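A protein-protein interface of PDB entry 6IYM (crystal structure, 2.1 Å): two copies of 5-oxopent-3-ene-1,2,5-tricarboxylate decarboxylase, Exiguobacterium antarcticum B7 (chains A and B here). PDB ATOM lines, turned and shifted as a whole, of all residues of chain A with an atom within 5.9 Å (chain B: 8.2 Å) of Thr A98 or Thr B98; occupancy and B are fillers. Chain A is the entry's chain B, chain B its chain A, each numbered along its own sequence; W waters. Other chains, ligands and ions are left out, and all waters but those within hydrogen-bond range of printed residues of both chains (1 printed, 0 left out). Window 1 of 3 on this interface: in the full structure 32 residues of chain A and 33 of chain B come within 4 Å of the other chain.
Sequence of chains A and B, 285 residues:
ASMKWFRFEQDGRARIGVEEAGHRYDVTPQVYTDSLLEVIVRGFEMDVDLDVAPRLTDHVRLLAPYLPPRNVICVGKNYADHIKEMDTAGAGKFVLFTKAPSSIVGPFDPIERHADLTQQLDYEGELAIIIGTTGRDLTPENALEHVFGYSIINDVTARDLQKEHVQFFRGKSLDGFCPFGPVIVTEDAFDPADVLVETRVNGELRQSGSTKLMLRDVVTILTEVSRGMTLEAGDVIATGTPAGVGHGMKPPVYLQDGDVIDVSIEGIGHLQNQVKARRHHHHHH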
ATOM      1  N   ASN A  71       3.614  13.116 -25.860  1.00  0.00           N
ATOM      2  CA  ASN A  71       3.846  12.649 -24.475  1.00  0.00           C
ATOM      3  C   ASN A  71       2.632  11.824 -24.038  1.00  0.00           C
ATOM      4  O   ASN A  71       1.493  12.185 -24.414  1.00  0.00           O
ATOM      5  CB  ASN A  71       4.088  13.804 -23.502  1.00  0.00           C
ATOM      6  CG  ASN A  71       5.367  14.568 -23.778  1.00  0.00           C
ATOM      7  OD1 ASN A  71       5.964  14.447 -24.838  1.00  0.00           O
ATOM      8  ND2 ASN A  71       5.827  15.298 -22.783  1.00  0.00           N
ATOM      9  N   VAL A  72       2.869  10.803 -23.230  1.00  0.00           N
ATOM     10  CA  VAL A  72       1.814  10.050 -22.484  1.00  0.00           C
ATOM     11  C   VAL A  72       1.125  11.028 -21.520  1.00  0.00           C
ATOM     12  O   VAL A  72       1.810  11.701 -20.752  1.00  0.00           O
ATOM     13  CB  VAL A  72       2.406   8.845 -21.737  1.00  0.00           C
ATOM     14  CG1 VAL A  72       1.333   8.042 -21.009  1.00  0.00           C
ATOM     15  CG2 VAL A  72       3.217   7.955 -22.670  1.00  0.00           C
ATOM     16  N   ILE A  73      -0.190  11.142 -21.613  1.00  0.00           N
ATOM     17  CA  ILE A  73      -1.030  12.007 -20.742  1.00  0.00           C
ATOM     18  C   ILE A  73      -1.376  11.172 -19.516  1.00  0.00           C
ATOM     19  O   ILE A  73      -1.831  10.011 -19.690  1.00  0.00           O
ATOM     20  CB  ILE A  73      -2.260  12.510 -21.518  1.00  0.00           C
ATOM     21  CG1 ILE A  73      -1.816  13.351 -22.720  1.00  0.00           C
ATOM     22  CG2 ILE A  73      -3.200  13.277 -20.586  1.00  0.00           C
ATOM     23  CD1 ILE A  73      -2.854  13.476 -23.862  1.00  0.00           C
ATOM     24  N   CYS A  74      -1.085  11.695 -18.330  1.00  0.00           N
ATOM     25  CA  CYS A  74      -1.165  10.936 -17.057  1.00  0.00           C
ATOM     26  C   CYS A  74      -2.102  11.644 -16.094  1.00  0.00           C
ATOM     27  O   CYS A  74      -2.024  12.878 -16.000  1.00  0.00           O
ATOM     28  CB  CYS A  74       0.210  10.809 -16.424  1.00  0.00           C
ATOM     29  SG  CYS A  74       1.385   9.862 -17.433  1.00  0.00           S
ATOM     30  N   LEU A  96      -3.540  16.601 -14.322  1.00  0.00           N
ATOM     31  CA  LEU A  96      -3.045  16.089 -15.637  1.00  0.00           C
ATOM     32  C   LEU A  96      -1.594  16.534 -15.862  1.00  0.00           C
ATOM     33  O   LEU A  96      -1.314  17.737 -15.738  1.00  0.00           O
ATOM     34  CB  LEU A  96      -3.929  16.636 -16.760  1.00  0.00           C
ATOM     35  CG  LEU A  96      -5.219  15.881 -17.063  1.00  0.00           C
ATOM     36  CD1 LEU A  96      -5.991  16.604 -18.153  1.00  0.00           C
ATOM     37  CD2 LEU A  96      -4.954  14.443 -17.485  1.00  0.00           C
ATOM     38  N   PHE A  97      -0.694  15.605 -16.174  1.00  0.00           N
ATOM     39  CA  PHE A  97       0.725  15.883 -16.515  1.00  0.00           C
ATOM     40  C   PHE A  97       1.131  14.876 -17.596  1.00  0.00           C
ATOM     41  O   PHE A  97       0.284  14.059 -17.965  1.00  0.00           O
ATOM     42  CB  PHE A  97       1.602  15.806 -15.261  1.00  0.00           C
ATOM     43  CG  PHE A  97       1.315  14.588 -14.430  1.00  0.00           C
ATOM     44  CD1 PHE A  97       0.298  14.608 -13.488  1.00  0.00           C
ATOM     45  CD2 PHE A  97       2.005  13.406 -14.652  1.00  0.00           C
ATOM     46  CE1 PHE A  97      -0.006  13.468 -12.764  1.00  0.00           C
ATOM     47  CE2 PHE A  97       1.705  12.276 -13.915  1.00  0.00           C
ATOM     48  CZ  PHE A  97       0.701  12.304 -12.976  1.00  0.00           C
ATOM     49  N   THR A  98       2.366  14.933 -18.092  1.00  0.00           N
ATOM     50  CA  THR A  98       2.809  14.069 -19.215  1.00  0.00           C
ATOM     51  C   THR A  98       4.113  13.360 -18.850  1.00  0.00           C
ATOM     52  O   THR A  98       4.801  13.803 -17.894  1.00  0.00           O
ATOM     53  CB  THR A  98       2.919  14.878 -20.511  1.00  0.00           C
ATOM     54  OG1 THR A  98       4.066  15.725 -20.434  1.00  0.00           O
ATOM     55  CG2 THR A  98       1.690  15.717 -20.807  1.00  0.00           C
ATOM     56  N   LYS A  99       4.419  12.291 -19.588  1.00  0.00           N
ATOM     57  CA  LYS A  99       5.735  11.607 -19.566  1.00  0.00           C
ATOM     58  C   LYS A  99       6.251  11.598 -20.995  1.00  0.00           C
ATOM     59  O   LYS A  99       5.438  11.288 -21.904  1.00  0.00           O
ATOM     60  CB  LYS A  99       5.647  10.186 -19.003  1.00  0.00           C
ATOM     61  CG  LYS A  99       4.962  10.030 -17.662  1.00  0.00           C
ATOM     62  CD  LYS A  99       4.630   8.575 -17.301  1.00  0.00           C
ATOM     63  CE  LYS A  99       5.868   7.692 -17.144  1.00  0.00           C
ATOM     64  NZ  LYS A  99       6.496   7.834 -15.797  1.00  0.00           N
ATOM     65  N   ALA A 100       7.519  11.974 -21.173  1.00  0.00           N
ATOM     66  CA  ALA A 100       8.203  11.992 -22.485  1.00  0.00           C
ATOM     67  C   ALA A 100       8.254  10.595 -23.098  1.00  0.00           C
ATOM     68  O   ALA A 100       8.583   9.629 -22.427  1.00  0.00           O
ATOM     69  CB  ALA A 100       9.586  12.563 -22.341  1.00  0.00           C
ATOM     70  N   PHE A 168       5.582  17.550 -12.312  1.00  0.00           N
ATOM     71  CA  PHE A 168       5.962  16.112 -12.258  1.00  0.00           C
ATOM     72  C   PHE A 168       6.752  15.654 -13.488  1.00  0.00           C
ATOM     73  O   PHE A 168       7.403  14.546 -13.404  1.00  0.00           O
ATOM     74  CB  PHE A 168       4.698  15.272 -12.094  1.00  0.00           C
ATOM     75  CG  PHE A 168       3.910  15.599 -10.855  1.00  0.00           C
ATOM     76  CD1 PHE A 168       4.450  16.382  -9.841  1.00  0.00           C
ATOM     77  CD2 PHE A 168       2.636  15.091 -10.686  1.00  0.00           C
ATOM     78  CE1 PHE A 168       3.717  16.669  -8.700  1.00  0.00           C
ATOM     79  CE2 PHE A 168       1.915  15.362  -9.539  1.00  0.00           C
ATOM     80  CZ  PHE A 168       2.456  16.146  -8.548  1.00  0.00           C
ATOM     81  N   PHE A 169       6.684  16.415 -14.587  1.00  0.00           N
ATOM     82  CA  PHE A 169       7.232  16.007 -15.909  1.00  0.00           C
ATOM     83  C   PHE A 169       8.626  15.395 -15.737  1.00  0.00           C
ATOM     84  O   PHE A 169       8.891  14.237 -16.184  1.00  0.00           O
ATOM     85  CB  PHE A 169       7.271  17.166 -16.897  1.00  0.00           C
ATOM     86  CG  PHE A 169       8.075  16.906 -18.150  1.00  0.00           C
ATOM     87  CD1 PHE A 169       7.644  15.985 -19.095  1.00  0.00           C
ATOM     88  CD2 PHE A 169       9.286  17.556 -18.368  1.00  0.00           C
ATOM     89  CE1 PHE A 169       8.370  15.765 -20.251  1.00  0.00           C
ATOM     90  CE2 PHE A 169      10.016  17.323 -19.523  1.00  0.00           C
ATOM     91  CZ  PHE A 169       9.552  16.438 -20.468  1.00  0.00           C
ATOM     92  N   LYS A 172       9.058  12.116 -13.789  1.00  0.00           N
ATOM     93  CA  LYS A 172       8.323  11.021 -14.448  1.00  0.00           C
ATOM     94  C   LYS A 172       8.871  10.722 -15.831  1.00  0.00           C
ATOM     95  O   LYS A 172       8.321   9.760 -16.443  1.00  0.00           O
ATOM     96  CB  LYS A 172       6.834  11.362 -14.487  1.00  0.00           C
ATOM     97  CG  LYS A 172       6.182  11.282 -13.109  1.00  0.00           C
ATOM     98  CD  LYS A 172       4.710  11.529 -13.108  1.00  0.00           C
ATOM     99  CE  LYS A 172       4.103  11.434 -11.722  1.00  0.00           C
ATOM    100  NZ  LYS A 172       3.686  10.049 -11.378  1.00  0.00           N
ATOM    101  N   SER A 173       9.896  11.436 -16.320  1.00  0.00           N
ATOM    102  CA  SER A 173      10.267  11.331 -17.756  1.00  0.00           C
ATOM    103  C   SER A 173      11.735  10.969 -17.967  1.00  0.00           C
ATOM    104  O   SER A 173      12.168  11.070 -19.136  1.00  0.00           O
ATOM    105  CB  SER A 173       9.882  12.572 -18.533  1.00  0.00           C
ATOM    106  OG  SER A 173       8.466  12.776 -18.473  1.00  0.00           O
ATOM    107  N   ARG B  70       7.194  15.797 -30.429  1.00  0.00           N
ATOM    108  CA  ARG B  70       6.742  15.534 -29.046  1.00  0.00           C
ATOM    109  C   ARG B  70       6.402  16.858 -28.349  1.00  0.00           C
ATOM    110  O   ARG B  70       6.620  17.918 -28.963  1.00  0.00           O
ATOM    111  CB  ARG B  70       7.780  14.627 -28.369  1.00  0.00           C
ATOM    112  CG  ARG B  70       9.027  15.310 -27.843  1.00  0.00           C
ATOM    113  CD  ARG B  70      10.037  14.212 -27.542  1.00  0.00           C
ATOM    114  NE  ARG B  70      11.225  14.682 -26.841  1.00  0.00           N
ATOM    115  CZ  ARG B  70      11.894  14.002 -25.907  1.00  0.00           C
ATOM    116  NH1 ARG B  70      11.488  12.805 -25.512  1.00  0.00           N
ATOM    117  NH2 ARG B  70      12.965  14.540 -25.358  1.00  0.00           N
ATOM    118  N   ASN B  71       5.860  16.815 -27.123  1.00  0.00           N
ATOM    119  CA  ASN B  71       5.365  18.052 -26.478  1.00  0.00           C
ATOM    120  C   ASN B  71       6.525  19.043 -26.408  1.00  0.00           C
ATOM    121  O   ASN B  71       7.682  18.621 -26.220  1.00  0.00           O
ATOM    122  CB  ASN B  71       4.817  17.862 -25.075  1.00  0.00           C
ATOM    123  CG  ASN B  71       3.588  16.984 -24.999  1.00  0.00           C
ATOM    124  OD1 ASN B  71       3.264  16.270 -25.933  1.00  0.00           O
ATOM    125  ND2 ASN B  71       2.934  16.998 -23.854  1.00  0.00           N
ATOM    126  N   VAL B  72       6.205  20.318 -26.597  1.00  0.00           N
ATOM    127  CA  VAL B  72       7.129  21.463 -26.361  1.00  0.00           C
ATOM    128  C   VAL B  72       7.503  21.461 -24.865  1.00  0.00           C
ATOM    129  O   VAL B  72       6.598  21.430 -23.998  1.00  0.00           O
ATOM    130  CB  VAL B  72       6.464  22.785 -26.788  1.00  0.00           C
ATOM    131  CG1 VAL B  72       7.357  23.972 -26.477  1.00  0.00           C
ATOM    132  CG2 VAL B  72       6.100  22.762 -28.261  1.00  0.00           C
ATOM    133  N   ILE B  73       8.795  21.412 -24.569  1.00  0.00           N
ATOM    134  CA  ILE B  73       9.300  21.420 -23.164  1.00  0.00           C
ATOM    135  C   ILE B  73       9.435  22.869 -22.729  1.00  0.00           C
ATOM    136  O   ILE B  73      10.092  23.608 -23.477  1.00  0.00           O
ATOM    137  CB  ILE B  73      10.630  20.662 -23.031  1.00  0.00           C
ATOM    138  CG1 ILE B  73      10.496  19.214 -23.519  1.00  0.00           C
ATOM    139  CG2 ILE B  73      11.137  20.753 -21.602  1.00  0.00           C
ATOM    140  CD1 ILE B  73      11.820  18.482 -23.735  1.00  0.00           C
ATOM    141  N   CYS B  74       8.844  23.225 -21.576  1.00  0.00           N
ATOM    142  CA  CYS B  74       8.699  24.615 -21.091  1.00  0.00           C
ATOM    143  C   CYS B  74       9.321  24.793 -19.703  1.00  0.00           C
ATOM    144  O   CYS B  74       9.061  23.973 -18.806  1.00  0.00           O
ATOM    145  CB  CYS B  74       7.228  24.999 -21.008  1.00  0.00           C
ATOM    146  SG  CYS B  74       6.399  25.030 -22.624  1.00  0.00           S
ATOM    147  N   VAL B  75      10.086  25.872 -19.550  1.00  0.00           N
ATOM    148  CA  VAL B  75      10.707  26.295 -18.273  1.00  0.00           C
ATOM    149  C   VAL B  75       9.719  27.202 -17.548  1.00  0.00           C
ATOM    150  O   VAL B  75       9.037  27.981 -18.232  1.00  0.00           O
ATOM    151  CB  VAL B  75      12.062  26.979 -18.530  1.00  0.00           C
ATOM    152  CG1 VAL B  75      12.687  27.481 -17.224  1.00  0.00           C
ATOM    153  CG2 VAL B  75      13.005  26.015 -19.239  1.00  0.00           C
ATOM    154  N   VAL B  95      11.763  24.573 -12.973  1.00  0.00           N
ATOM    155  CA  VAL B  95      10.384  24.047 -13.155  1.00  0.00           C
ATOM    156  C   VAL B  95      10.264  23.679 -14.636  1.00  0.00           C
ATOM    157  O   VAL B  95      10.717  24.505 -15.482  1.00  0.00           O
ATOM    158  CB  VAL B  95       9.336  25.093 -12.710  1.00  0.00           C
ATOM    159  CG1 VAL B  95       7.914  24.713 -13.089  1.00  0.00           C
ATOM    160  CG2 VAL B  95       9.412  25.361 -11.213  1.00  0.00           C
ATOM    161  N   LEU B  96       9.788  22.461 -14.931  1.00  0.00           N
ATOM    162  CA  LEU B  96       9.655  21.945 -16.317  1.00  0.00           C
ATOM    163  C   LEU B  96       8.241  21.407 -16.494  1.00  0.00           C
ATOM    164  O   LEU B  96       7.798  20.736 -15.615  1.00  0.00           O
ATOM    165  CB  LEU B  96      10.693  20.853 -16.585  1.00  0.00           C
ATOM    166  CG  LEU B  96      12.098  21.361 -16.898  1.00  0.00           C
ATOM    167  CD1 LEU B  96      13.108  20.221 -16.941  1.00  0.00           C
ATOM    168  CD2 LEU B  96      12.125  22.129 -18.216  1.00  0.00           C
ATOM    169  N   PHE B  97       7.568  21.755 -17.590  1.00  0.00           N
ATOM    170  CA  PHE B  97       6.236  21.217 -17.980  1.00  0.00           C
ATOM    171  C   PHE B  97       6.137  21.243 -19.510  1.00  0.00           C
ATOM    172  O   PHE B  97       7.082  21.740 -20.178  1.00  0.00           O
ATOM    173  CB  PHE B  97       5.118  22.018 -17.314  1.00  0.00           C
ATOM    174  CG  PHE B  97       5.297  23.494 -17.493  1.00  0.00           C
ATOM    175  CD1 PHE B  97       6.036  24.226 -16.584  1.00  0.00           C
ATOM    176  CD2 PHE B  97       4.766  24.132 -18.600  1.00  0.00           C
ATOM    177  CE1 PHE B  97       6.227  25.586 -16.765  1.00  0.00           C
ATOM    178  CE2 PHE B  97       4.967  25.489 -18.786  1.00  0.00           C
ATOM    179  CZ  PHE B  97       5.696  26.212 -17.870  1.00  0.00           C
ATOM    180  N   THR B  98       5.039  20.737 -20.076  1.00  0.00           N
ATOM    181  CA  THR B  98       4.934  20.613 -21.549  1.00  0.00           C
ATOM    182  C   THR B  98       3.646  21.238 -22.075  1.00  0.00           C
ATOM    183  O   THR B  98       2.696  21.514 -21.290  1.00  0.00           O
ATOM    184  CB  THR B  98       5.058  19.141 -21.949  1.00  0.00           C
ATOM    185  OG1 THR B  98       3.894  18.432 -21.520  1.00  0.00           O
ATOM    186  CG2 THR B  98       6.305  18.517 -21.381  1.00  0.00           C
ATOM    187  N   LYS B  99       3.627  21.416 -23.386  1.00  0.00           N
ATOM    188  CA  LYS B  99       2.444  21.839 -24.172  1.00  0.00           C
ATOM    189  C   LYS B  99       2.218  20.805 -25.269  1.00  0.00           C
ATOM    190  O   LYS B  99       3.176  20.556 -25.993  1.00  0.00           O
ATOM    191  CB  LYS B  99       2.693  23.205 -24.804  1.00  0.00           C
ATOM    192  CG  LYS B  99       2.742  24.353 -23.805  1.00  0.00           C
ATOM    193  CD  LYS B  99       3.274  25.604 -24.432  1.00  0.00           C
ATOM    194  CE  LYS B  99       2.185  26.425 -25.100  1.00  0.00           C
ATOM    195  NZ  LYS B  99       1.300  27.069 -24.090  1.00  0.00           N
ATOM    196  N   ALA B 100       1.020  20.215 -25.343  1.00  0.00           N
ATOM    197  CA  ALA B 100       0.628  19.259 -26.406  1.00  0.00           C
ATOM    198  C   ALA B 100       0.899  19.911 -27.753  1.00  0.00           C
ATOM    199  O   ALA B 100       0.673  21.114 -27.889  1.00  0.00           O
ATOM    200  CB  ALA B 100      -0.810  18.854 -26.284  1.00  0.00           C
ATOM    201  N   PRO B 101       1.444  19.149 -28.737  1.00  0.00           N
ATOM    202  CA  PRO B 101       1.650  19.635 -30.102  1.00  0.00           C
ATOM    203  C   PRO B 101       0.350  20.069 -30.807  1.00  0.00           C
ATOM    204  O   PRO B 101       0.390  20.923 -31.618  1.00  0.00           O
ATOM    205  CB  PRO B 101       2.204  18.412 -30.845  1.00  0.00           C
ATOM    206  CG  PRO B 101       2.801  17.547 -29.785  1.00  0.00           C
ATOM    207  CD  PRO B 101       1.923  17.769 -28.570  1.00  0.00           C
ATOM    208  N   SER B 103      -1.610  22.048 -29.719  1.00  0.00           N
ATOM    209  CA  SER B 103      -1.825  23.486 -29.351  1.00  0.00           C
ATOM    210  C   SER B 103      -1.089  24.442 -30.291  1.00  0.00           C
ATOM    211  O   SER B 103      -1.423  25.653 -30.267  1.00  0.00           O
ATOM    212  CB  SER B 103      -1.483  23.779 -27.919  1.00  0.00           C
ATOM    213  OG  SER B 103      -0.080  23.770 -27.701  1.00  0.00           O
ATOM    214  N   ASP B 155       3.770  31.126 -25.060  1.00  0.00           N
ATOM    215  CA  ASP B 155       3.277  30.098 -24.108  1.00  0.00           C
ATOM    216  C   ASP B 155       1.940  30.616 -23.610  1.00  0.00           C
ATOM    217  O   ASP B 155       1.864  31.053 -22.458  1.00  0.00           O
ATOM    218  CB  ASP B 155       4.314  29.815 -23.002  1.00  0.00           C
ATOM    219  CG  ASP B 155       3.881  28.876 -21.870  1.00  0.00           C
ATOM    220  OD1 ASP B 155       2.837  28.215 -22.001  1.00  0.00           O
ATOM    221  OD2 ASP B 155       4.595  28.825 -20.823  1.00  0.00           O
ATOM    222  N   GLN B 167      -1.292  20.892 -12.041  1.00  0.00           N
ATOM    223  CA  GLN B 167      -0.155  20.816 -12.987  1.00  0.00           C
ATOM    224  C   GLN B 167      -0.483  21.703 -14.181  1.00  0.00           C
ATOM    225  O   GLN B 167      -1.656  21.800 -14.502  1.00  0.00           O
ATOM    226  CB  GLN B 167       0.074  19.370 -13.403  1.00  0.00           C
ATOM    227  CG  GLN B 167       0.415  18.498 -12.220  1.00  0.00           C
ATOM    228  CD  GLN B 167       1.869  18.596 -11.878  1.00  0.00           C
ATOM    229  OE1 GLN B 167       2.736  18.456 -12.749  1.00  0.00           O
ATOM    230  NE2 GLN B 167       2.135  18.815 -10.600  1.00  0.00           N
ATOM    231  N   PHE B 168       0.522  22.342 -14.789  1.00  0.00           N
ATOM    232  CA  PHE B 168       0.299  23.433 -15.777  1.00  0.00           C
ATOM    233  C   PHE B 168      -0.201  22.882 -17.122  1.00  0.00           C
ATOM    234  O   PHE B 168      -0.810  23.663 -17.869  1.00  0.00           O
ATOM    235  CB  PHE B 168       1.560  24.291 -15.900  1.00  0.00           C
ATOM    236  CG  PHE B 168       1.937  25.035 -14.645  1.00  0.00           C
ATOM    237  CD1 PHE B 168       1.044  25.187 -13.598  1.00  0.00           C
ATOM    238  CD2 PHE B 168       3.186  25.609 -14.534  1.00  0.00           C
ATOM    239  CE1 PHE B 168       1.408  25.864 -12.445  1.00  0.00           C
ATOM    240  CE2 PHE B 168       3.547  26.301 -13.391  1.00  0.00           C
ATOM    241  CZ  PHE B 168       2.655  26.430 -12.348  1.00  0.00           C
ATOM    242  N   PHE B 169      -0.018  21.584 -17.388  1.00  0.00           N
ATOM    243  CA  PHE B 169      -0.193  20.919 -18.705  1.00  0.00           C
ATOM    244  C   PHE B 169      -1.480  21.353 -19.406  1.00  0.00           C
ATOM    245  O   PHE B 169      -1.407  21.866 -20.523  1.00  0.00           O
ATOM    246  CB  PHE B 169      -0.269  19.396 -18.567  1.00  0.00           C
ATOM    247  CG  PHE B 169      -0.622  18.714 -19.864  1.00  0.00           C
ATOM    248  CD1 PHE B 169       0.197  18.834 -20.967  1.00  0.00           C
ATOM    249  CD2 PHE B 169      -1.781  17.975 -19.986  1.00  0.00           C
ATOM    250  CE1 PHE B 169      -0.136  18.210 -22.158  1.00  0.00           C
ATOM    251  CE2 PHE B 169      -2.104  17.346 -21.173  1.00  0.00           C
ATOM    252  CZ  PHE B 169      -1.291  17.471 -22.257  1.00  0.00           C
ATOM    253  N   ARG B 170      -2.629  21.112 -18.787  1.00  0.00           N
ATOM    254  CA  ARG B 170      -3.951  21.345 -19.415  1.00  0.00           C
ATOM    255  C   ARG B 170      -4.114  22.839 -19.734  1.00  0.00           C
ATOM    256  O   ARG B 170      -4.455  23.138 -20.866  1.00  0.00           O
ATOM    257  CB  ARG B 170      -5.113  20.847 -18.546  1.00  0.00           C
ATOM    258  CG  ARG B 170      -6.462  21.074 -19.212  1.00  0.00           C
ATOM    259  CD  ARG B 170      -7.588  20.143 -18.777  1.00  0.00           C
ATOM    260  NE  ARG B 170      -8.857  20.773 -19.119  1.00  0.00           N
ATOM    261  CZ  ARG B 170      -9.365  20.831 -20.335  1.00  0.00           C
ATOM    262  NH1 ARG B 170      -8.748  20.281 -21.369  1.00  0.00           N
ATOM    263  NH2 ARG B 170     -10.508  21.455 -20.526  1.00  0.00           N
ATOM    264  N   GLY B 171      -3.900  23.723 -18.765  1.00  0.00           N
ATOM    265  CA  GLY B 171      -4.104  25.176 -18.938  1.00  0.00           C
ATOM    266  C   GLY B 171      -3.155  25.782 -19.964  1.00  0.00           C
ATOM    267  O   GLY B 171      -3.411  26.934 -20.357  1.00  0.00           O
ATOM    268  N   LYS B 172      -2.129  25.039 -20.421  1.00  0.00           N
ATOM    269  CA  LYS B 172      -1.149  25.511 -21.443  1.00  0.00           C
ATOM    270  C   LYS B 172      -1.349  24.794 -22.781  1.00  0.00           C
ATOM    271  O   LYS B 172      -0.613  25.113 -23.725  1.00  0.00           O
ATOM    272  CB  LYS B 172       0.274  25.352 -20.903  1.00  0.00           C
ATOM    273  CG  LYS B 172       0.569  26.323 -19.768  1.00  0.00           C
ATOM    274  CD  LYS B 172       1.961  26.338 -19.230  1.00  0.00           C
ATOM    275  CE  LYS B 172       2.171  27.449 -18.210  1.00  0.00           C
ATOM    276  NZ  LYS B 172       2.705  28.703 -18.805  1.00  0.00           N
ATOM    277  N   SER B 173      -2.311  23.873 -22.872  1.00  0.00           N
ATOM    278  CA  SER B 173      -2.357  22.868 -23.953  1.00  0.00           C
ATOM    279  C   SER B 173      -3.678  22.870 -24.734  1.00  0.00           C
ATOM    280  O   SER B 173      -3.786  22.057 -25.693  1.00  0.00           O
ATOM    281  CB  SER B 173      -2.015  21.518 -23.384  1.00  0.00           C
ATOM    282  OG  SER B 173      -0.693  21.537 -22.883  1.00  0.00           O
ATOM    283  N   CYS B 178      -0.247  27.624 -28.521  1.00  0.00           N
ATOM    284  CA  CYS B 178       1.219  27.628 -28.774  1.00  0.00           C
ATOM    285  C   CYS B 178       1.568  28.180 -30.154  1.00  0.00           C
ATOM    286  O   CYS B 178       2.081  27.461 -31.015  1.00  0.00           O
ATOM    287  CB  CYS B 178       1.804  26.233 -28.548  1.00  0.00           C
ATOM    288  SG  CYS B 178       3.588  26.281 -28.259  1.00  0.00           S
ATOM    289  N   MET B 229      17.737  12.335 -19.266  1.00  0.00           N
ATOM    290  CA  MET B 229      16.620  12.423 -20.258  1.00  0.00           C
ATOM    291  C   MET B 229      17.169  12.767 -21.644  1.00  0.00           C
ATOM    292  O   MET B 229      17.733  13.876 -21.805  1.00  0.00           O
ATOM    293  CB  MET B 229      15.575  13.470 -19.876  1.00  0.00           C
ATOM    294  CG  MET B 229      14.273  13.232 -20.634  1.00  0.00           C
ATOM    295  SD  MET B 229      13.031  14.508 -20.348  1.00  0.00           S
ATOM    296  CE  MET B 229      13.801  15.906 -21.148  1.00  0.00           C
ATOM    297  N   VAL B 236      11.634  21.225 -29.093  1.00  0.00           N
ATOM    298  CA  VAL B 236      11.447  22.694 -28.901  1.00  0.00           C
ATOM    299  C   VAL B 236      11.465  22.968 -27.397  1.00  0.00           C
ATOM    300  O   VAL B 236      10.587  22.470 -26.676  1.00  0.00           O
ATOM    301  CB  VAL B 236      10.142  23.210 -29.539  1.00  0.00           C
ATOM    302  CG1 VAL B 236       9.985  24.721 -29.396  1.00  0.00           C
ATOM    303  CG2 VAL B 236      10.035  22.827 -31.000  1.00  0.00           C
HETATM  304  O   HOH W   1       4.153  18.155 -15.166  1.00  0.00           O
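Of the 25 printed residues of chain B, 8 touch a printed residue of chain A.
Printed residues of chain B that touch a printed residue of chain A: Arg B70, Asn B71, Leu B96, Thr B98, Gln B167, Phe B169, Arg B170 and Met B229.
Hydrophobic or aromatic side chains of chain B within 4 Å of the printed part of chain A: Phe B169 and Met B229.
Of the 13 printed residues of chain A, 8 touch a printed residue of chain B.
Among the printed residues, 16 pairs touch across the chains.
Among the printed residues, no Asp or Glu carboxylate lies within 4 Å of a Lys or Arg side-chain nitrogen of the other chain.
Asn A71 touches Thr B98, and with the chains exchanged Thr A98 touches Asn B71.
Leu A96 touches Phe B169, and with the chains exchanged Phe A169 touches Leu B96.
Positions printed for both chains: 71, 72, 73, 74, 96, 97, 98, 99, 100, 168, 169, 172 and 173.
The side-chain sulfur (SD) of Met B229 sits close to the backbone carbonyl oxygen (O) of Ser A173, 3.7 Å away.
The side-chain amide oxygen (OE1) of Gln B167 lies within hydrogen-bond range of the backbone NH (N) of Phe A168.
OG1 of Thr B98 lies within hydrogen-bond range of OG1 of Thr A98, 2.9 Å away.
N of Asn A71 sits at hydrogen-bond distance from OD1 of Asn B71.
Water W1 lies within hydrogen-bond range of the side-chain amide oxygen (OE1) of Gln B167 (2.8 Å), the backbone NH (N) of Phe A169 (3.1 Å) and the backbone NH (N) of Phe A168 (3.2 Å).
Of chain B, only Asn B71 (3.5 Å), Thr B98 (2.9 Å) and Phe B169 (3.4 Å) come within 4 Å of Thr A98.
Of the printed residues of chain A, Arg B170 touches Leu A96 (3.9 Å).
Of the printed residues of chain A, Leu B96 touches Phe A169 (3.8 Å).
Of the printed residues of chain A, Gln B167 touches Leu A96 (3.2 Å), Phe A97 (3.8 Å) and Phe A168 (3.0 Å).
Val B236 touches none of the printed residues of chain A.
Ala B100 touches none of the printed residues of chain A.
The nearest printed residue of chain A that does not touch Thr B98 is Phe A97 (6.0 Å).
The nearest printed residue of chain A that does not touch Gln B167 is Phe A169 (4.8 Å).
ND2 of Asn A71 touches CG2 of Thr B98, 3.5 Å away.
Gln B167 touches Leu A96 (CB to O, 3.2 Å).
Leu A96 touches Phe B169 (O to CB, 3.4 Å).
CD of Arg B170 touches CD1 of Leu A96, 3.9 Å away.
CG2 of Thr A98 touches ND2 of Asn B71 (3.5 Å).
CG2 of Thr A98 touches CE1 of Phe B169 (3.4 Å).
Arg B70 touches Ala A100.
Phe A169 touches Leu B96 (CB to O, 3.8 Å).
Phe A169 touches Met B229.
OG of Ser A173 sits at hydrogen-bond distance from N of Ala A100, 3.0 Å away.
The side-chain hydroxyl (OG1) of Thr B98 sits at hydrogen-bond distance from the side-chain amide nitrogen (ND2) of Asn B71, 2.9 Å away.
O of Phe A169 lies within hydrogen-bond range of OG of Ser A173, 2.7 Å away.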
